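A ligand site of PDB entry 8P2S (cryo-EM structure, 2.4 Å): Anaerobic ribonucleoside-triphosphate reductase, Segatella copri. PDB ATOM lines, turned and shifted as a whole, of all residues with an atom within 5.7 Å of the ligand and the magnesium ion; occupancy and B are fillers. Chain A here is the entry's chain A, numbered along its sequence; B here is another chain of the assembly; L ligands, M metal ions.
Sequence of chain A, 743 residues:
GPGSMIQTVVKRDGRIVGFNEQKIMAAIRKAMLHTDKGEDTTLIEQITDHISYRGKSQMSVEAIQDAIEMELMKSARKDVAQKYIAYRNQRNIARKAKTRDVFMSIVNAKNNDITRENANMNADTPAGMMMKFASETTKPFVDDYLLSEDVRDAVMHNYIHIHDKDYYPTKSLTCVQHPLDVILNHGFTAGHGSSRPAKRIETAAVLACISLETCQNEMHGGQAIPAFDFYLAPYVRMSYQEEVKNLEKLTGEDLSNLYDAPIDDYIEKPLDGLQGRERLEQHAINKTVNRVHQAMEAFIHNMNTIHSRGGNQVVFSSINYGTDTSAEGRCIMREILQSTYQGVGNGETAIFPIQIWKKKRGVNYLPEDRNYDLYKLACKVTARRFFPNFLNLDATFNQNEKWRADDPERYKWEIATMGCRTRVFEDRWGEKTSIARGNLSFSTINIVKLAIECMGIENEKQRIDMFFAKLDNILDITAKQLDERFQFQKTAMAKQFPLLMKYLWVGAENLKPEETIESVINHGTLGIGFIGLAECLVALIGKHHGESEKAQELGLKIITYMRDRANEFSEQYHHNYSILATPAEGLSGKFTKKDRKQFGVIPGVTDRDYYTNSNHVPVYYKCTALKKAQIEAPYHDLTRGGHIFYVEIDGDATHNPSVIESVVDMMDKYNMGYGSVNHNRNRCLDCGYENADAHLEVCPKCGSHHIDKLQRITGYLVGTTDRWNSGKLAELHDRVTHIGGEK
An oxygen (O9) of the ligand is bound to the magnesium ion, at 2.1 Å.
An oxygen (O5) of the ligand binds the magnesium ion, at 2.3 Å.
The magnesium ion has two donor atoms within binding distance.
Slightly farther from the magnesium ion lies an oxygen (O2) of the ligand (2.6 Å).
Slightly farther from the magnesium ion lies OE1 of Glu 297 of chain B (2.8 Å).
O2 of the ligand lies within salt-bridge range of NH2 of Arg 200 (2.7 Å).
N2 of the ligand is in hydrogen-bond range of OD1 of Asn 302 of chain B (3.1 Å).
An oxygen (O12) of the ligand sits at hydrogen-bond distance from the backbone NH (N) of Arg 196 (3.1 Å).
An oxygen (O4) of the ligand is in salt-bridge range of the guanidinium group (NE) of Arg 196, at 3.2 Å.
An oxygen (O12) of the ligand lies within hydrogen-bond range of a ring nitrogen (NE2) of His 301 of chain B (3.2 Å).
OG1 of Thr 203 lies within hydrogen-bond range of O11 of the ligand (3.3 Å).
N of Lys 199 sits at hydrogen-bond distance from O1 of the ligand.
The side-chain carboxylate of Glu 242 is in salt-bridge range of the guanidinium group of Arg 200 (2.8 Å).
A ring nitrogen (ND1) of His 301 of chain B lies within hydrogen-bond range of the backbone carbonyl oxygen of Glu 297 of chain B.
NE2 of Gln 294 of chain B sits at hydrogen-bond distance from OD1 of Asn 290 of chain B (2.8 Å).
ND2 of Asn 302 of chain B lies close to O of Ala 298 of chain B (3.4 Å).
The backbone carbonyl oxygen (O) of Gly 345 of chain B lies within hydrogen-bond range of the guanidinium group (NH1) of Arg 196 (2.9 Å).
NE2 of His 301 of chain B sits at hydrogen-bond distance from N of Gly 345 of chain B (3.4 Å).
O of His 301 of chain B is in hydrogen-bond range of OG1 of Thr 305 of chain B (2.9 Å).
The side-chain amino group of Lys 199 lies within hydrogen-bond range of the backbone carbonyl oxygen of Pro 197 (3.0 Å).
NH2 of Arg 200 touches the magnesium ion, 3.4 Å away.
OE1 of Gln 294 of chain B touches the magnesium ion (2.9 Å).
Of the 23 residues printed, 3 come within 4 Å of the magnesium ion.
The nearest printed residue that does not touch the magnesium ion is His 293 of chain B (4.6 Å).
OG of Ser 195 touches O13 of the ligand, 3.96 Å away.
Pro 197 touches the ligand (O to C1, 3.5 Å).
Val 206 of chain A touches the ligand (CG1 to O14, 3.2 Å).
Leu 207 touches the ligand.
Gln 294 of chain B touches the ligand (OE1 to O9, 3.9 Å).
Ala 298 of chain B touches the ligand.
Along chain A the residues within 4 Å of the ligand span positions 195 to 207.
The nearest printed residue that does not touch the ligand is Ala 198 (4.05 Å).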
ATOM      1  N   SER A 194      -8.046 -26.922  14.246  1.00  0.00           N
ATOM      2  CA  SER A 194      -8.653 -25.628  14.484  1.00  0.00           C
ATOM      3  C   SER A 194      -7.713 -24.525  14.007  1.00  0.00           C
ATOM      4  O   SER A 194      -6.523 -24.548  14.331  1.00  0.00           O
ATOM      5  CB  SER A 194      -8.980 -25.439  15.972  1.00  0.00           C
ATOM      6  OG  SER A 194      -7.837 -25.648  16.773  1.00  0.00           O
ATOM      7  N   SER A 195      -8.259 -23.584  13.250  1.00  0.00           N
ATOM      8  CA  SER A 195      -7.512 -22.435  12.760  1.00  0.00           C
ATOM      9  C   SER A 195      -8.228 -21.143  13.113  1.00  0.00           C
ATOM     10  O   SER A 195      -9.453 -21.036  12.958  1.00  0.00           O
ATOM     11  CB  SER A 195      -7.301 -22.503  11.247  1.00  0.00           C
ATOM     12  OG  SER A 195      -6.587 -23.675  10.885  1.00  0.00           O
ATOM     13  N   ARG A 196      -7.467 -20.174  13.589  1.00  0.00           N
ATOM     14  CA  ARG A 196      -7.963 -18.861  13.950  1.00  0.00           C
ATOM     15  C   ARG A 196      -8.218 -18.029  12.697  1.00  0.00           C
ATOM     16  O   ARG A 196      -7.763 -18.386  11.602  1.00  0.00           O
ATOM     17  CB  ARG A 196      -6.964 -18.172  14.880  1.00  0.00           C
ATOM     18  CG  ARG A 196      -6.828 -18.835  16.235  1.00  0.00           C
ATOM     19  CD  ARG A 196      -5.967 -18.031  17.180  1.00  0.00           C
ATOM     20  NE  ARG A 196      -4.596 -17.888  16.691  1.00  0.00           N
ATOM     21  CZ  ARG A 196      -3.612 -18.716  17.007  1.00  0.00           C
ATOM     22  NH1 ARG A 196      -3.803 -19.763  17.780  1.00  0.00           N
ATOM     23  NH2 ARG A 196      -2.395 -18.470  16.523  1.00  0.00           N
ATOM     24  N   PRO A 197      -8.969 -16.932  12.810  1.00  0.00           N
ATOM     25  CA  PRO A 197      -9.185 -16.068  11.644  1.00  0.00           C
ATOM     26  C   PRO A 197      -7.876 -15.543  11.071  1.00  0.00           C
ATOM     27  O   PRO A 197      -6.930 -15.237  11.812  1.00  0.00           O
ATOM     28  CB  PRO A 197     -10.049 -14.927  12.213  1.00  0.00           C
ATOM     29  CG  PRO A 197     -10.758 -15.544  13.357  1.00  0.00           C
ATOM     30  CD  PRO A 197      -9.792 -16.519  13.964  1.00  0.00           C
ATOM     31  N   ALA A 198      -7.831 -15.441   9.747  1.00  0.00           N
ATOM     32  CA  ALA A 198      -6.618 -15.005   9.067  1.00  0.00           C
ATOM     33  C   ALA A 198      -6.310 -13.546   9.361  1.00  0.00           C
ATOM     34  O   ALA A 198      -7.207 -12.729   9.614  1.00  0.00           O
ATOM     35  CB  ALA A 198      -6.766 -15.214   7.558  1.00  0.00           C
ATOM     36  N   LYS A 199      -5.013 -13.215   9.319  1.00  0.00           N
ATOM     37  CA  LYS A 199      -4.543 -11.853   9.552  1.00  0.00           C
ATOM     38  C   LYS A 199      -3.636 -11.369   8.436  1.00  0.00           C
ATOM     39  O   LYS A 199      -3.060 -10.283   8.541  1.00  0.00           O
ATOM     40  CB  LYS A 199      -3.810 -11.762  10.896  1.00  0.00           C
ATOM     41  CG  LYS A 199      -4.655 -12.133  12.103  1.00  0.00           C
ATOM     42  CD  LYS A 199      -5.726 -11.096  12.363  1.00  0.00           C
ATOM     43  CE  LYS A 199      -6.529 -11.462  13.598  1.00  0.00           C
ATOM     44  NZ  LYS A 199      -7.245 -12.759  13.425  1.00  0.00           N
ATOM     45  N   ARG A 200      -3.507 -12.125   7.359  1.00  0.00           N
ATOM     46  CA  ARG A 200      -2.558 -11.829   6.293  1.00  0.00           C
ATOM     47  C   ARG A 200      -3.008 -12.524   5.019  1.00  0.00           C
ATOM     48  O   ARG A 200      -3.909 -13.367   5.025  1.00  0.00           O
ATOM     49  CB  ARG A 200      -1.142 -12.265   6.662  1.00  0.00           C
ATOM     50  CG  ARG A 200      -0.312 -11.225   7.375  1.00  0.00           C
ATOM     51  CD  ARG A 200       0.971 -11.835   7.910  1.00  0.00           C
ATOM     52  NE  ARG A 200       0.712 -12.890   8.888  1.00  0.00           N
ATOM     53  CZ  ARG A 200       0.452 -12.669  10.174  1.00  0.00           C
ATOM     54  NH1 ARG A 200       0.404 -11.447  10.670  1.00  0.00           N
ATOM     55  NH2 ARG A 200       0.233 -13.705  10.973  1.00  0.00           N
ATOM     56  N   GLU A 202      -0.730 -14.310   3.356  1.00  0.00           N
ATOM     57  CA  GLU A 202      -0.016 -15.583   3.435  1.00  0.00           C
ATOM     58  C   GLU A 202      -0.851 -16.636   4.138  1.00  0.00           C
ATOM     59  O   GLU A 202      -0.892 -17.793   3.701  1.00  0.00           O
ATOM     60  CB  GLU A 202       1.321 -15.387   4.151  1.00  0.00           C
ATOM     61  CG  GLU A 202       2.319 -14.506   3.409  1.00  0.00           C
ATOM     62  CD  GLU A 202       2.096 -13.029   3.650  1.00  0.00           C
ATOM     63  OE1 GLU A 202       1.134 -12.678   4.364  1.00  0.00           O
ATOM     64  OE2 GLU A 202       2.882 -12.214   3.125  1.00  0.00           O
ATOM     65  N   THR A 203      -1.512 -16.262   5.237  1.00  0.00           N
ATOM     66  CA  THR A 203      -2.380 -17.209   5.918  1.00  0.00           C
ATOM     67  C   THR A 203      -3.703 -17.399   5.183  1.00  0.00           C
ATOM     68  O   THR A 203      -4.291 -18.485   5.248  1.00  0.00           O
ATOM     69  CB  THR A 203      -2.630 -16.763   7.356  1.00  0.00           C
ATOM     70  OG1 THR A 203      -3.622 -17.609   7.953  1.00  0.00           O
ATOM     71  CG2 THR A 203      -3.086 -15.336   7.405  1.00  0.00           C
ATOM     72  N   VAL A 206      -3.204 -20.004   2.420  1.00  0.00           N
ATOM     73  CA  VAL A 206      -3.046 -21.331   3.002  1.00  0.00           C
ATOM     74  C   VAL A 206      -4.369 -21.841   3.539  1.00  0.00           C
ATOM     75  O   VAL A 206      -4.676 -23.029   3.444  1.00  0.00           O
ATOM     76  CB  VAL A 206      -1.957 -21.311   4.084  1.00  0.00           C
ATOM     77  CG1 VAL A 206      -1.855 -22.667   4.756  1.00  0.00           C
ATOM     78  CG2 VAL A 206      -0.620 -20.937   3.470  1.00  0.00           C
ATOM     79  N   LEU A 207      -5.187 -20.952   4.117  1.00  0.00           N
ATOM     80  CA  LEU A 207      -6.512 -21.365   4.578  1.00  0.00           C
ATOM     81  C   LEU A 207      -7.425 -21.746   3.418  1.00  0.00           C
ATOM     82  O   LEU A 207      -8.231 -22.666   3.544  1.00  0.00           O
ATOM     83  CB  LEU A 207      -7.147 -20.267   5.423  1.00  0.00           C
ATOM     84  CG  LEU A 207      -6.582 -20.064   6.828  1.00  0.00           C
ATOM     85  CD1 LEU A 207      -7.406 -19.054   7.604  1.00  0.00           C
ATOM     86  CD2 LEU A 207      -6.500 -21.376   7.581  1.00  0.00           C
ATOM     87  N   ILE A 210      -6.309 -25.149   2.489  1.00  0.00           N
ATOM     88  CA  ILE A 210      -6.739 -26.099   3.513  1.00  0.00           C
ATOM     89  C   ILE A 210      -8.219 -26.410   3.384  1.00  0.00           C
ATOM     90  O   ILE A 210      -8.638 -27.568   3.492  1.00  0.00           O
ATOM     91  CB  ILE A 210      -6.407 -25.544   4.909  1.00  0.00           C
ATOM     92  CG1 ILE A 210      -4.908 -25.674   5.197  1.00  0.00           C
ATOM     93  CG2 ILE A 210      -7.223 -26.237   5.973  1.00  0.00           C
ATOM     94  CD1 ILE A 210      -4.407 -27.107   5.168  1.00  0.00           C
ATOM     95  N   GLU A 242       0.078  -3.947   8.015  1.00  0.00           N
ATOM     96  CA  GLU A 242       1.239  -4.492   8.727  1.00  0.00           C
ATOM     97  C   GLU A 242       2.534  -3.857   8.242  1.00  0.00           C
ATOM     98  O   GLU A 242       3.413  -3.533   9.040  1.00  0.00           O
ATOM     99  CB  GLU A 242       1.290  -6.011   8.566  1.00  0.00           C
ATOM    100  CG  GLU A 242       0.166  -6.750   9.264  1.00  0.00           C
ATOM    101  CD  GLU A 242       0.346  -8.248   9.215  1.00  0.00           C
ATOM    102  OE1 GLU A 242       1.360  -8.703   8.648  1.00  0.00           O
ATOM    103  OE2 GLU A 242      -0.527  -8.975   9.731  1.00  0.00           O
ATOM    104  N   VAL B 206       6.619 -24.600   4.805  1.00  0.00           N
ATOM    105  CA  VAL B 206       5.569 -25.156   3.961  1.00  0.00           C
ATOM    106  C   VAL B 206       6.105 -26.318   3.146  1.00  0.00           C
ATOM    107  O   VAL B 206       5.397 -27.307   2.934  1.00  0.00           O
ATOM    108  CB  VAL B 206       4.949 -24.066   3.073  1.00  0.00           C
ATOM    109  CG1 VAL B 206       3.900 -24.669   2.160  1.00  0.00           C
ATOM    110  CG2 VAL B 206       4.348 -22.966   3.923  1.00  0.00           C
ATOM    111  N   ASN B 290       9.895 -12.640  14.021  1.00  0.00           N
ATOM    112  CA  ASN B 290       8.475 -12.700  13.673  1.00  0.00           C
ATOM    113  C   ASN B 290       8.251 -13.614  12.478  1.00  0.00           C
ATOM    114  O   ASN B 290       7.344 -14.454  12.491  1.00  0.00           O
ATOM    115  CB  ASN B 290       7.938 -11.308  13.393  1.00  0.00           C
ATOM    116  CG  ASN B 290       6.430 -11.261  13.332  1.00  0.00           C
ATOM    117  OD1 ASN B 290       5.746 -12.103  13.932  1.00  0.00           O
ATOM    118  ND2 ASN B 290       5.883 -10.290  12.606  1.00  0.00           N
ATOM    119  N   HIS B 293       8.282 -16.914  13.798  1.00  0.00           N
ATOM    120  CA  HIS B 293       7.182 -17.277  14.686  1.00  0.00           C
ATOM    121  C   HIS B 293       5.944 -17.725  13.929  1.00  0.00           C
ATOM    122  O   HIS B 293       5.274 -18.656  14.387  1.00  0.00           O
ATOM    123  CB  HIS B 293       6.820 -16.092  15.583  1.00  0.00           C
ATOM    124  CG  HIS B 293       5.674 -16.376  16.509  1.00  0.00           C
ATOM    125  ND1 HIS B 293       5.691 -17.406  17.418  1.00  0.00           N
ATOM    126  CD2 HIS B 293       4.474 -15.770  16.644  1.00  0.00           C
ATOM    127  CE1 HIS B 293       4.549 -17.411  18.087  1.00  0.00           C
ATOM    128  NE2 HIS B 293       3.789 -16.433  17.636  1.00  0.00           N
ATOM    129  N   GLN B 294       5.647 -17.112  12.792  1.00  0.00           N
ATOM    130  CA  GLN B 294       4.544 -17.579  11.957  1.00  0.00           C
ATOM    131  C   GLN B 294       4.890 -18.914  11.294  1.00  0.00           C
ATOM    132  O   GLN B 294       4.105 -19.873  11.368  1.00  0.00           O
ATOM    133  CB  GLN B 294       4.199 -16.530  10.908  1.00  0.00           C
ATOM    134  CG  GLN B 294       3.206 -15.467  11.359  1.00  0.00           C
ATOM    135  CD  GLN B 294       3.782 -14.535  12.401  1.00  0.00           C
ATOM    136  OE1 GLN B 294       3.745 -14.831  13.592  1.00  0.00           O
ATOM    137  NE2 GLN B 294       4.314 -13.407  11.953  1.00  0.00           N
ATOM    138  N   GLU B 297       4.518 -21.562  13.738  1.00  0.00           N
ATOM    139  CA  GLU B 297       3.121 -21.694  14.117  1.00  0.00           C
ATOM    140  C   GLU B 297       2.325 -22.367  13.015  1.00  0.00           C
ATOM    141  O   GLU B 297       1.625 -23.359  13.255  1.00  0.00           O
ATOM    142  CB  GLU B 297       2.533 -20.318  14.431  1.00  0.00           C
ATOM    143  CG  GLU B 297       1.031 -20.291  14.597  1.00  0.00           C
ATOM    144  CD  GLU B 297       0.485 -18.882  14.712  1.00  0.00           C
ATOM    145  OE1 GLU B 297       1.294 -17.925  14.633  1.00  0.00           O
ATOM    146  OE2 GLU B 297      -0.739 -18.725  14.870  1.00  0.00           O
ATOM    147  N   ALA B 298       2.464 -21.879  11.785  1.00  0.00           N
ATOM    148  CA  ALA B 298       1.830 -22.510  10.637  1.00  0.00           C
ATOM    149  C   ALA B 298       2.130 -24.000  10.604  1.00  0.00           C
ATOM    150  O   ALA B 298       1.218 -24.823  10.468  1.00  0.00           O
ATOM    151  CB  ALA B 298       2.304 -21.845   9.346  1.00  0.00           C
ATOM    152  N   HIS B 301       0.180 -25.820  13.064  1.00  0.00           N
ATOM    153  CA  HIS B 301      -1.210 -25.894  12.633  1.00  0.00           C
ATOM    154  C   HIS B 301      -1.370 -26.851  11.462  1.00  0.00           C
ATOM    155  O   HIS B 301      -2.270 -27.694  11.469  1.00  0.00           O
ATOM    156  CB  HIS B 301      -1.724 -24.501  12.269  1.00  0.00           C
ATOM    157  CG  HIS B 301      -2.061 -23.665  13.456  1.00  0.00           C
ATOM    158  ND1 HIS B 301      -1.106 -23.066  14.242  1.00  0.00           N
ATOM    159  CD2 HIS B 301      -3.262 -23.344  14.007  1.00  0.00           C
ATOM    160  CE1 HIS B 301      -1.700 -22.405  15.221  1.00  0.00           C
ATOM    161  NE2 HIS B 301      -2.999 -22.553  15.102  1.00  0.00           N
ATOM    162  N   ASN B 302      -0.470 -26.775  10.476  1.00  0.00           N
ATOM    163  CA  ASN B 302      -0.653 -27.582   9.274  1.00  0.00           C
ATOM    164  C   ASN B 302      -0.611 -29.076   9.595  1.00  0.00           C
ATOM    165  O   ASN B 302      -1.490 -29.826   9.141  1.00  0.00           O
ATOM    166  CB  ASN B 302       0.394 -27.229   8.227  1.00  0.00           C
ATOM    167  CG  ASN B 302       0.148 -25.876   7.587  1.00  0.00           C
ATOM    168  OD1 ASN B 302      -0.982 -25.391   7.575  1.00  0.00           O
ATOM    169  ND2 ASN B 302       1.196 -25.273   7.052  1.00  0.00           N
ATOM    170  N   THR B 305      -3.738 -30.059  11.012  1.00  0.00           N
ATOM    171  CA  THR B 305      -4.869 -29.965  10.094  1.00  0.00           C
ATOM    172  C   THR B 305      -4.816 -31.013   8.992  1.00  0.00           C
ATOM    173  O   THR B 305      -5.795 -31.737   8.786  1.00  0.00           O
ATOM    174  CB  THR B 305      -4.944 -28.574   9.465  1.00  0.00           C
ATOM    175  OG1 THR B 305      -5.042 -27.594  10.504  1.00  0.00           O
ATOM    176  CG2 THR B 305      -6.161 -28.470   8.573  1.00  0.00           C
ATOM    177  N   GLY B 345      -5.397 -23.105  17.416  1.00  0.00           N
ATOM    178  CA  GLY B 345      -6.775 -22.644  17.442  1.00  0.00           C
ATOM    179  C   GLY B 345      -7.025 -21.784  18.664  1.00  0.00           C
ATOM    180  O   GLY B 345      -6.244 -20.882  18.992  1.00  0.00           O
HETATM  181  P1  LIG L   1      -2.303 -15.873  11.659  1.00  0.00           P
HETATM  182  O1  LIG L   1      -2.514 -14.870  10.557  1.00  0.00           O
HETATM  183  O2  LIG L   1      -0.833 -15.993  11.987  1.00  0.00           O
HETATM  184  O3  LIG L   1      -3.188 -15.507  12.950  1.00  0.00           O
HETATM  185  P2  LIG L   1      -2.554 -14.987  14.331  1.00  0.00           P
HETATM  186  O4  LIG L   1      -3.569 -15.157  15.436  1.00  0.00           O
HETATM  187  O5  LIG L   1      -1.276 -15.711  14.667  1.00  0.00           O
HETATM  188  O6  LIG L   1      -2.312 -13.432  14.038  1.00  0.00           O
HETATM  189  P3  LIG L   1      -1.057 -12.643  14.674  1.00  0.00           P
HETATM  190  O7  LIG L   1      -1.156 -12.663  16.179  1.00  0.00           O
HETATM  191  O8  LIG L   1      -1.077 -11.226  14.184  1.00  0.00           O
HETATM  192  O9  LIG L   1       0.217 -13.309  14.235  1.00  0.00           O
HETATM  193  O10 LIG L   1      -2.913 -17.296  11.243  1.00  0.00           O
HETATM  194  C1  LIG L   1      -4.328 -17.509  11.275  1.00  0.00           C
HETATM  195  C2  LIG L   1      -4.555 -18.988  11.548  1.00  0.00           C
HETATM  196  O11 LIG L   1      -4.250 -19.725  10.374  1.00  0.00           O
HETATM  197  C3  LIG L   1      -3.608 -19.461  12.640  1.00  0.00           C
HETATM  198  O12 LIG L   1      -4.339 -19.924  13.782  1.00  0.00           O
HETATM  199  C4  LIG L   1      -2.806 -20.597  12.049  1.00  0.00           C
HETATM  200  C5  LIG L   1      -3.419 -20.848  10.677  1.00  0.00           C
HETATM  201  N1  LIG L   1      -2.390 -20.972   9.658  1.00  0.00           N
HETATM  202  C6  LIG L   1      -2.264 -22.183   8.965  1.00  0.00           C
HETATM  203  O13 LIG L   1      -3.030 -23.129   9.236  1.00  0.00           O
HETATM  204  N2  LIG L   1      -1.334 -22.354   8.014  1.00  0.00           N
HETATM  205  C7  LIG L   1      -0.501 -21.358   7.699  1.00  0.00           C
HETATM  206  O14 LIG L   1       0.366 -21.515   6.814  1.00  0.00           O
HETATM  207  C8  LIG L   1      -0.613 -20.066   8.417  1.00  0.00           C
HETATM  208  C9  LIG L   1       0.311 -18.933   8.092  1.00  0.00           C
HETATM  209  C10 LIG L   1      -1.585 -19.934   9.401  1.00  0.00           C
HETATM  210 MG    MG M   1       0.864 -15.289  13.876  1.00  0.00          MG
